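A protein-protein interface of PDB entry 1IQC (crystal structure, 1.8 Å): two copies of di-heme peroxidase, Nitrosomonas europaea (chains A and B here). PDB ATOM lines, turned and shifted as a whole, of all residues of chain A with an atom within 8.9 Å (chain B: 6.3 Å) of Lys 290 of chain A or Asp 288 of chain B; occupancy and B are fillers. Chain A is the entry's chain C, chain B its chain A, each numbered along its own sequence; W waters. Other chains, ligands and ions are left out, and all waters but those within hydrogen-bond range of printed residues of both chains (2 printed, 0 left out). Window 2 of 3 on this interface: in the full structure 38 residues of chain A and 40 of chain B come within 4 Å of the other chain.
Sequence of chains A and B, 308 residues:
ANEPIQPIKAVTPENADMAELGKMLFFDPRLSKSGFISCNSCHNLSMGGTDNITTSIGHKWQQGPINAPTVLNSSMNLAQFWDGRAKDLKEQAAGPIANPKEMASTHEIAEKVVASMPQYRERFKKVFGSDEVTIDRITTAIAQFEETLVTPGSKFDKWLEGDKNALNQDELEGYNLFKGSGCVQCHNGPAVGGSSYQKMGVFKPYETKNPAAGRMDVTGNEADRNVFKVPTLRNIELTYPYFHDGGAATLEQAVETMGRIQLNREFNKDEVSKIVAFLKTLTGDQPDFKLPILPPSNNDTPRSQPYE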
ATOM      1  N   GLU A  20     -28.045  -6.185  12.969  1.00  0.00           N
ATOM      2  CA  GLU A  20     -26.715  -6.780  13.001  1.00  0.00           C
ATOM      3  C   GLU A  20     -26.704  -7.981  13.939  1.00  0.00           C
ATOM      4  O   GLU A  20     -26.076  -9.001  13.646  1.00  0.00           O
ATOM      5  CB  GLU A  20     -25.674  -5.758  13.454  1.00  0.00           C
ATOM      6  CG  GLU A  20     -25.150  -4.878  12.332  1.00  0.00           C
ATOM      7  CD  GLU A  20     -24.546  -5.689  11.197  1.00  0.00           C
ATOM      8  OE1 GLU A  20     -23.686  -6.553  11.473  1.00  0.00           O
ATOM      9  OE2 GLU A  20     -24.926  -5.460  10.030  1.00  0.00           O
ATOM     10  N   LYS A  23     -28.441 -10.711  12.195  1.00  0.00           N
ATOM     11  CA  LYS A  23     -27.596 -11.305  11.159  1.00  0.00           C
ATOM     12  C   LYS A  23     -26.700 -12.369  11.777  1.00  0.00           C
ATOM     13  O   LYS A  23     -26.590 -13.481  11.261  1.00  0.00           O
ATOM     14  CB  LYS A  23     -26.717 -10.244  10.499  1.00  0.00           C
ATOM     15  CG  LYS A  23     -25.831 -10.789   9.383  1.00  0.00           C
ATOM     16  CD  LYS A  23     -24.868  -9.731   8.859  1.00  0.00           C
ATOM     17  CE  LYS A  23     -25.601  -8.491   8.364  1.00  0.00           C
ATOM     18  NZ  LYS A  23     -24.678  -7.329   8.143  1.00  0.00           N
ATOM     19  N   MET A  24     -26.046 -12.015  12.877  1.00  0.00           N
ATOM     20  CA  MET A  24     -25.155 -12.940  13.570  1.00  0.00           C
ATOM     21  C   MET A  24     -25.876 -14.224  13.983  1.00  0.00           C
ATOM     22  O   MET A  24     -25.385 -15.334  13.744  1.00  0.00           O
ATOM     23  CB  MET A  24     -24.550 -12.246  14.792  1.00  0.00           C
ATOM     24  CG  MET A  24     -23.634 -11.095  14.422  1.00  0.00           C
ATOM     25  SD  MET A  24     -23.042 -10.168  15.851  1.00  0.00           S
ATOM     26  CE  MET A  24     -22.002 -11.438  16.636  1.00  0.00           C
ATOM     27  N   PHE A  27     -26.663 -16.702  11.233  1.00  0.00           N
ATOM     28  CA  PHE A  27     -25.507 -17.484  10.786  1.00  0.00           C
ATOM     29  C   PHE A  27     -24.861 -18.333  11.874  1.00  0.00           C
ATOM     30  O   PHE A  27     -23.879 -19.026  11.611  1.00  0.00           O
ATOM     31  CB  PHE A  27     -24.418 -16.571  10.208  1.00  0.00           C
ATOM     32  CG  PHE A  27     -24.692 -16.097   8.810  1.00  0.00           C
ATOM     33  CD1 PHE A  27     -25.584 -15.050   8.574  1.00  0.00           C
ATOM     34  CD2 PHE A  27     -24.036 -16.686   7.729  1.00  0.00           C
ATOM     35  CE1 PHE A  27     -25.818 -14.593   7.279  1.00  0.00           C
ATOM     36  CE2 PHE A  27     -24.256 -16.246   6.432  1.00  0.00           C
ATOM     37  CZ  PHE A  27     -25.154 -15.188   6.198  1.00  0.00           C
ATOM     38  N   PHE A 145     -33.489  -8.545  11.025  1.00  0.00           N
ATOM     39  CA  PHE A 145     -32.490  -8.809   9.995  1.00  0.00           C
ATOM     40  C   PHE A 145     -33.187  -9.261   8.713  1.00  0.00           C
ATOM     41  O   PHE A 145     -32.853  -8.807   7.617  1.00  0.00           O
ATOM     42  CB  PHE A 145     -31.510  -9.895  10.464  1.00  0.00           C
ATOM     43  CG  PHE A 145     -30.639 -10.443   9.361  1.00  0.00           C
ATOM     44  CD1 PHE A 145     -29.746  -9.619   8.677  1.00  0.00           C
ATOM     45  CD2 PHE A 145     -30.723 -11.788   9.005  1.00  0.00           C
ATOM     46  CE1 PHE A 145     -28.944 -10.124   7.646  1.00  0.00           C
ATOM     47  CE2 PHE A 145     -29.928 -12.307   7.977  1.00  0.00           C
ATOM     48  CZ  PHE A 145     -29.037 -11.477   7.295  1.00  0.00           C
ATOM     49  N   PRO A 287     -28.111 -10.156  -1.087  1.00  0.00           N
ATOM     50  CA  PRO A 287     -27.580  -9.602   0.163  1.00  0.00           C
ATOM     51  C   PRO A 287     -26.130  -9.165   0.025  1.00  0.00           C
ATOM     52  O   PRO A 287     -25.276  -9.933  -0.415  1.00  0.00           O
ATOM     53  CB  PRO A 287     -27.754 -10.755   1.151  1.00  0.00           C
ATOM     54  CG  PRO A 287     -28.989 -11.422   0.652  1.00  0.00           C
ATOM     55  CD  PRO A 287     -28.738 -11.468  -0.841  1.00  0.00           C
ATOM     56  N   ASP A 288     -25.866  -7.920   0.409  1.00  0.00           N
ATOM     57  CA  ASP A 288     -24.537  -7.335   0.323  1.00  0.00           C
ATOM     58  C   ASP A 288     -24.058  -6.926   1.710  1.00  0.00           C
ATOM     59  O   ASP A 288     -24.393  -5.843   2.197  1.00  0.00           O
ATOM     60  CB  ASP A 288     -24.585  -6.105  -0.591  1.00  0.00           C
ATOM     61  CG  ASP A 288     -23.241  -5.419  -0.730  1.00  0.00           C
ATOM     62  OD1 ASP A 288     -23.206  -4.303  -1.295  1.00  0.00           O
ATOM     63  OD2 ASP A 288     -22.219  -5.987  -0.285  1.00  0.00           O
ATOM     64  N   PHE A 289     -23.295  -7.804   2.353  1.00  0.00           N
ATOM     65  CA  PHE A 289     -22.765  -7.509   3.678  1.00  0.00           C
ATOM     66  C   PHE A 289     -21.564  -8.389   3.986  1.00  0.00           C
ATOM     67  O   PHE A 289     -21.341  -9.407   3.328  1.00  0.00           O
ATOM     68  CB  PHE A 289     -23.855  -7.662   4.754  1.00  0.00           C
ATOM     69  CG  PHE A 289     -24.522  -9.015   4.788  1.00  0.00           C
ATOM     70  CD1 PHE A 289     -23.831 -10.148   5.208  1.00  0.00           C
ATOM     71  CD2 PHE A 289     -25.864  -9.148   4.438  1.00  0.00           C
ATOM     72  CE1 PHE A 289     -24.472 -11.391   5.281  1.00  0.00           C
ATOM     73  CE2 PHE A 289     -26.510 -10.381   4.508  1.00  0.00           C
ATOM     74  CZ  PHE A 289     -25.813 -11.503   4.931  1.00  0.00           C
ATOM     75  N   LYS A 290     -20.775  -7.976   4.970  1.00  0.00           N
ATOM     76  CA  LYS A 290     -19.591  -8.728   5.354  1.00  0.00           C
ATOM     77  C   LYS A 290     -19.971 -10.039   6.024  1.00  0.00           C
ATOM     78  O   LYS A 290     -20.970 -10.114   6.735  1.00  0.00           O
ATOM     79  CB  LYS A 290     -18.741  -7.909   6.329  1.00  0.00           C
ATOM     80  CG  LYS A 290     -18.209  -6.600   5.770  1.00  0.00           C
ATOM     81  CD  LYS A 290     -17.184  -6.845   4.687  1.00  0.00           C
ATOM     82  CE  LYS A 290     -16.497  -5.552   4.267  1.00  0.00           C
ATOM     83  NZ  LYS A 290     -15.502  -5.795   3.188  1.00  0.00           N
ATOM     84  N   LEU A 291     -19.169 -11.072   5.789  1.00  0.00           N
ATOM     85  CA  LEU A 291     -19.407 -12.361   6.424  1.00  0.00           C
ATOM     86  C   LEU A 291     -19.382 -12.084   7.928  1.00  0.00           C
ATOM     87  O   LEU A 291     -18.407 -11.547   8.450  1.00  0.00           O
ATOM     88  CB  LEU A 291     -18.284 -13.334   6.075  1.00  0.00           C
ATOM     89  CG  LEU A 291     -18.372 -14.696   6.763  1.00  0.00           C
ATOM     90  CD1 LEU A 291     -19.530 -15.466   6.166  1.00  0.00           C
ATOM     91  CD2 LEU A 291     -17.061 -15.451   6.585  1.00  0.00           C
ATOM     92  N   PRO A 292     -20.455 -12.437   8.645  1.00  0.00           N
ATOM     93  CA  PRO A 292     -20.435 -12.170  10.085  1.00  0.00           C
ATOM     94  C   PRO A 292     -19.375 -12.954  10.854  1.00  0.00           C
ATOM     95  O   PRO A 292     -19.151 -14.135  10.594  1.00  0.00           O
ATOM     96  CB  PRO A 292     -21.856 -12.519  10.522  1.00  0.00           C
ATOM     97  CG  PRO A 292     -22.280 -13.556   9.539  1.00  0.00           C
ATOM     98  CD  PRO A 292     -21.744 -13.024   8.229  1.00  0.00           C
ATOM     99  N   ILE A 293     -18.718 -12.275  11.789  1.00  0.00           N
ATOM    100  CA  ILE A 293     -17.697 -12.893  12.629  1.00  0.00           C
ATOM    101  C   ILE A 293     -18.379 -13.082  13.977  1.00  0.00           C
ATOM    102  O   ILE A 293     -18.789 -12.114  14.623  1.00  0.00           O
ATOM    103  CB  ILE A 293     -16.452 -11.983  12.755  1.00  0.00           C
ATOM    104  CG1 ILE A 293     -15.834 -11.762  11.372  1.00  0.00           C
ATOM    105  CG2 ILE A 293     -15.428 -12.613  13.688  1.00  0.00           C
ATOM    106  CD1 ILE A 293     -15.437 -13.046  10.641  1.00  0.00           C
ATOM    107  N   LYS B  23     -12.514 -18.090  -3.263  1.00  0.00           N
ATOM    108  CA  LYS B  23     -13.450 -17.761  -2.192  1.00  0.00           C
ATOM    109  C   LYS B  23     -14.844 -18.290  -2.530  1.00  0.00           C
ATOM    110  O   LYS B  23     -15.521 -18.881  -1.687  1.00  0.00           O
ATOM    111  CB  LYS B  23     -13.510 -16.244  -2.004  1.00  0.00           C
ATOM    112  CG  LYS B  23     -14.478 -15.787  -0.922  1.00  0.00           C
ATOM    113  CD  LYS B  23     -14.673 -14.270  -0.947  1.00  0.00           C
ATOM    114  CE  LYS B  23     -13.351 -13.528  -0.845  1.00  0.00           C
ATOM    115  NZ  LYS B  23     -13.522 -12.049  -1.008  1.00  0.00           N
ATOM    116  N   GLN B 286      -9.997 -11.611  12.139  1.00  0.00           N
ATOM    117  CA  GLN B 286     -10.701 -12.623  11.372  1.00  0.00           C
ATOM    118  C   GLN B 286     -10.978 -12.145   9.949  1.00  0.00           C
ATOM    119  O   GLN B 286     -10.960 -10.945   9.671  1.00  0.00           O
ATOM    120  CB  GLN B 286     -11.998 -12.993  12.091  1.00  0.00           C
ATOM    121  CG  GLN B 286     -11.739 -13.552  13.482  1.00  0.00           C
ATOM    122  CD  GLN B 286     -10.783 -14.732  13.454  1.00  0.00           C
ATOM    123  OE1 GLN B 286     -11.079 -15.768  12.857  1.00  0.00           O
ATOM    124  NE2 GLN B 286      -9.624 -14.578  14.100  1.00  0.00           N
ATOM    125  N   PRO B 287     -11.245 -13.086   9.030  1.00  0.00           N
ATOM    126  CA  PRO B 287     -11.521 -12.758   7.630  1.00  0.00           C
ATOM    127  C   PRO B 287     -12.522 -11.620   7.497  1.00  0.00           C
ATOM    128  O   PRO B 287     -13.572 -11.623   8.140  1.00  0.00           O
ATOM    129  CB  PRO B 287     -12.060 -14.069   7.068  1.00  0.00           C
ATOM    130  CG  PRO B 287     -11.342 -15.103   7.887  1.00  0.00           C
ATOM    131  CD  PRO B 287     -11.448 -14.525   9.275  1.00  0.00           C
ATOM    132  N   ASP B 288     -12.180 -10.648   6.662  1.00  0.00           N
ATOM    133  CA  ASP B 288     -13.043  -9.501   6.434  1.00  0.00           C
ATOM    134  C   ASP B 288     -13.343  -9.367   4.953  1.00  0.00           C
ATOM    135  O   ASP B 288     -12.560  -8.793   4.201  1.00  0.00           O
ATOM    136  CB  ASP B 288     -12.372  -8.223   6.940  1.00  0.00           C
ATOM    137  CG  ASP B 288     -13.112  -6.970   6.514  1.00  0.00           C
ATOM    138  OD1 ASP B 288     -14.338  -6.891   6.734  1.00  0.00           O
ATOM    139  OD2 ASP B 288     -12.459  -6.058   5.961  1.00  0.00           O
ATOM    140  N   PHE B 289     -14.477  -9.918   4.537  1.00  0.00           N
ATOM    141  CA  PHE B 289     -14.892  -9.849   3.144  1.00  0.00           C
ATOM    142  C   PHE B 289     -16.401 -10.033   3.027  1.00  0.00           C
ATOM    143  O   PHE B 289     -17.058 -10.496   3.958  1.00  0.00           O
ATOM    144  CB  PHE B 289     -14.139 -10.891   2.303  1.00  0.00           C
ATOM    145  CG  PHE B 289     -14.268 -12.306   2.802  1.00  0.00           C
ATOM    146  CD1 PHE B 289     -15.480 -12.987   2.715  1.00  0.00           C
ATOM    147  CD2 PHE B 289     -13.167 -12.969   3.335  1.00  0.00           C
ATOM    148  CE1 PHE B 289     -15.594 -14.301   3.146  1.00  0.00           C
ATOM    149  CE2 PHE B 289     -13.270 -14.290   3.770  1.00  0.00           C
ATOM    150  CZ  PHE B 289     -14.488 -14.957   3.675  1.00  0.00           C
ATOM    151  N   LYS B 290     -16.951  -9.646   1.886  1.00  0.00           N
ATOM    152  CA  LYS B 290     -18.382  -9.758   1.663  1.00  0.00           C
ATOM    153  C   LYS B 290     -18.802 -11.209   1.490  1.00  0.00           C
ATOM    154  O   LYS B 290     -18.066 -12.007   0.915  1.00  0.00           O
ATOM    155  CB  LYS B 290     -18.784  -8.988   0.400  1.00  0.00           C
ATOM    156  CG  LYS B 290     -18.526  -7.489   0.454  1.00  0.00           C
ATOM    157  CD  LYS B 290     -19.396  -6.819   1.505  1.00  0.00           C
ATOM    158  CE  LYS B 290     -19.259  -5.300   1.439  1.00  0.00           C
ATOM    159  NZ  LYS B 290     -19.643  -4.787   0.093  1.00  0.00           N
ATOM    160  N   LEU B 291     -19.990 -11.539   1.986  1.00  0.00           N
ATOM    161  CA  LEU B 291     -20.521 -12.885   1.830  1.00  0.00           C
ATOM    162  C   LEU B 291     -20.536 -13.164   0.324  1.00  0.00           C
ATOM    163  O   LEU B 291     -21.096 -12.396  -0.458  1.00  0.00           O
ATOM    164  CB  LEU B 291     -21.946 -12.957   2.377  1.00  0.00           C
ATOM    165  CG  LEU B 291     -22.662 -14.301   2.209  1.00  0.00           C
ATOM    166  CD1 LEU B 291     -22.067 -15.320   3.163  1.00  0.00           C
ATOM    167  CD2 LEU B 291     -24.155 -14.118   2.469  1.00  0.00           C
HETATM  168  O   HOH W   1     -16.044 -10.563   7.431  1.00  0.00           O
HETATM  169  O   HOH W   2     -22.649 -10.106   0.058  1.00  0.00           O
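Printed residues of chain B that touch a printed residue of chain A: Gln 286, Pro 287, Asp 288, Phe 289, Lys 290 and Leu 291. Along chain B the printed residues that touch a printed residue of chain A span positions 286 to 291. Of the 12 printed residues of chain A, 5 touch a printed residue of chain B. Among the printed residues, Asp or Glu carboxylates within 4 Å of a Lys or Arg side-chain nitrogen of the other chain: Asp 288 of chain A with Lys 290 of chain B (2.9 Å) and Lys 290 of chain A with Asp 288 of chain B (3.9 Å).
Lys 290 of chain A touches three residues of chain B. Asp 288 of chain B touches one residue of chain A. Of the printed residues of chain B, Leu 291 of chain A touches Phe 289 (2.9 Å) and Leu 291 (3.9 Å). Printed residues of chain A within 4 Å of Phe 289 of chain B: Lys 290 (3.4 Å) and Leu 291 (2.9 Å). Pro 287 of chain A touches none of the printed residues of chain B. Pro 292 of chain A touches none of the printed residues of chain B. The nearest printed residue of chain A that does not touch Gln 286 of chain B is Pro 292 of chain A (7.4 Å).
The side-chain carboxylate (OD1) of Asp 288 of chain B is in salt-bridge range of the side-chain amino group (NZ) of Lys 290 of chain A (3.9 Å). The backbone carbonyl oxygen of Phe 289 of chain B lies within hydrogen-bond range of the backbone NH of Leu 291 of chain A, 2.9 Å away. NZ of Lys 290 of chain B is in salt-bridge range of OD2 of Asp 288 of chain A, at 2.9 Å. N of Leu 291 of chain B is in hydrogen-bond range of O of Phe 289 of chain A.
Among the printed residues, merely in contact across the chains: Lys 290 of chain A with Phe 289 of chain B (3.4 Å), Phe 289 of chain A with Lys 290 of chain B (3.4 Å), Ile 293 of chain A with Pro 287 of chain B (3.4 Å), Ile 293 of chain A with Gln 286 of chain B (3.7 Å), Lys 290 of chain A with Lys 290 of chain B (3.9 Å) and Leu 291 of chain A with Leu 291 of chain B (3.9 Å).
Asp 288 of chain A touches Lys 290 of chain B, and with the chains exchanged Lys 290 of chain A touches Asp 288 of chain B. Phe 289 of chain A touches Lys 290 of chain B, and with the chains exchanged Lys 290 of chain A touches Phe 289 of chain B. Lys 290 of chain B touches its own counterpart, Lys 290 of chain A. Leu 291 of chain B touches its own counterpart, Leu 291 of chain A. 6 positions are printed for both chains. Of the 10 pairs that touch across the chains among the printed residues, 8 have their exchanged pair printed and touching as well.
Water W2 lies within hydrogen-bond range of the backbone carbonyl oxygen (O) of Pro 287 of chain A (2.7 Å), the backbone carbonyl oxygen (O) of Leu 291 of chain B (2.8 Å) and the backbone NH (N) of Phe 289 of chain A (3.3 Å). Water W1 lies within hydrogen-bond range of the backbone carbonyl oxygen of Leu 291 of chain A, the backbone carbonyl oxygen of Pro 287 of chain B and the backbone NH of Phe 289 of chain B.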
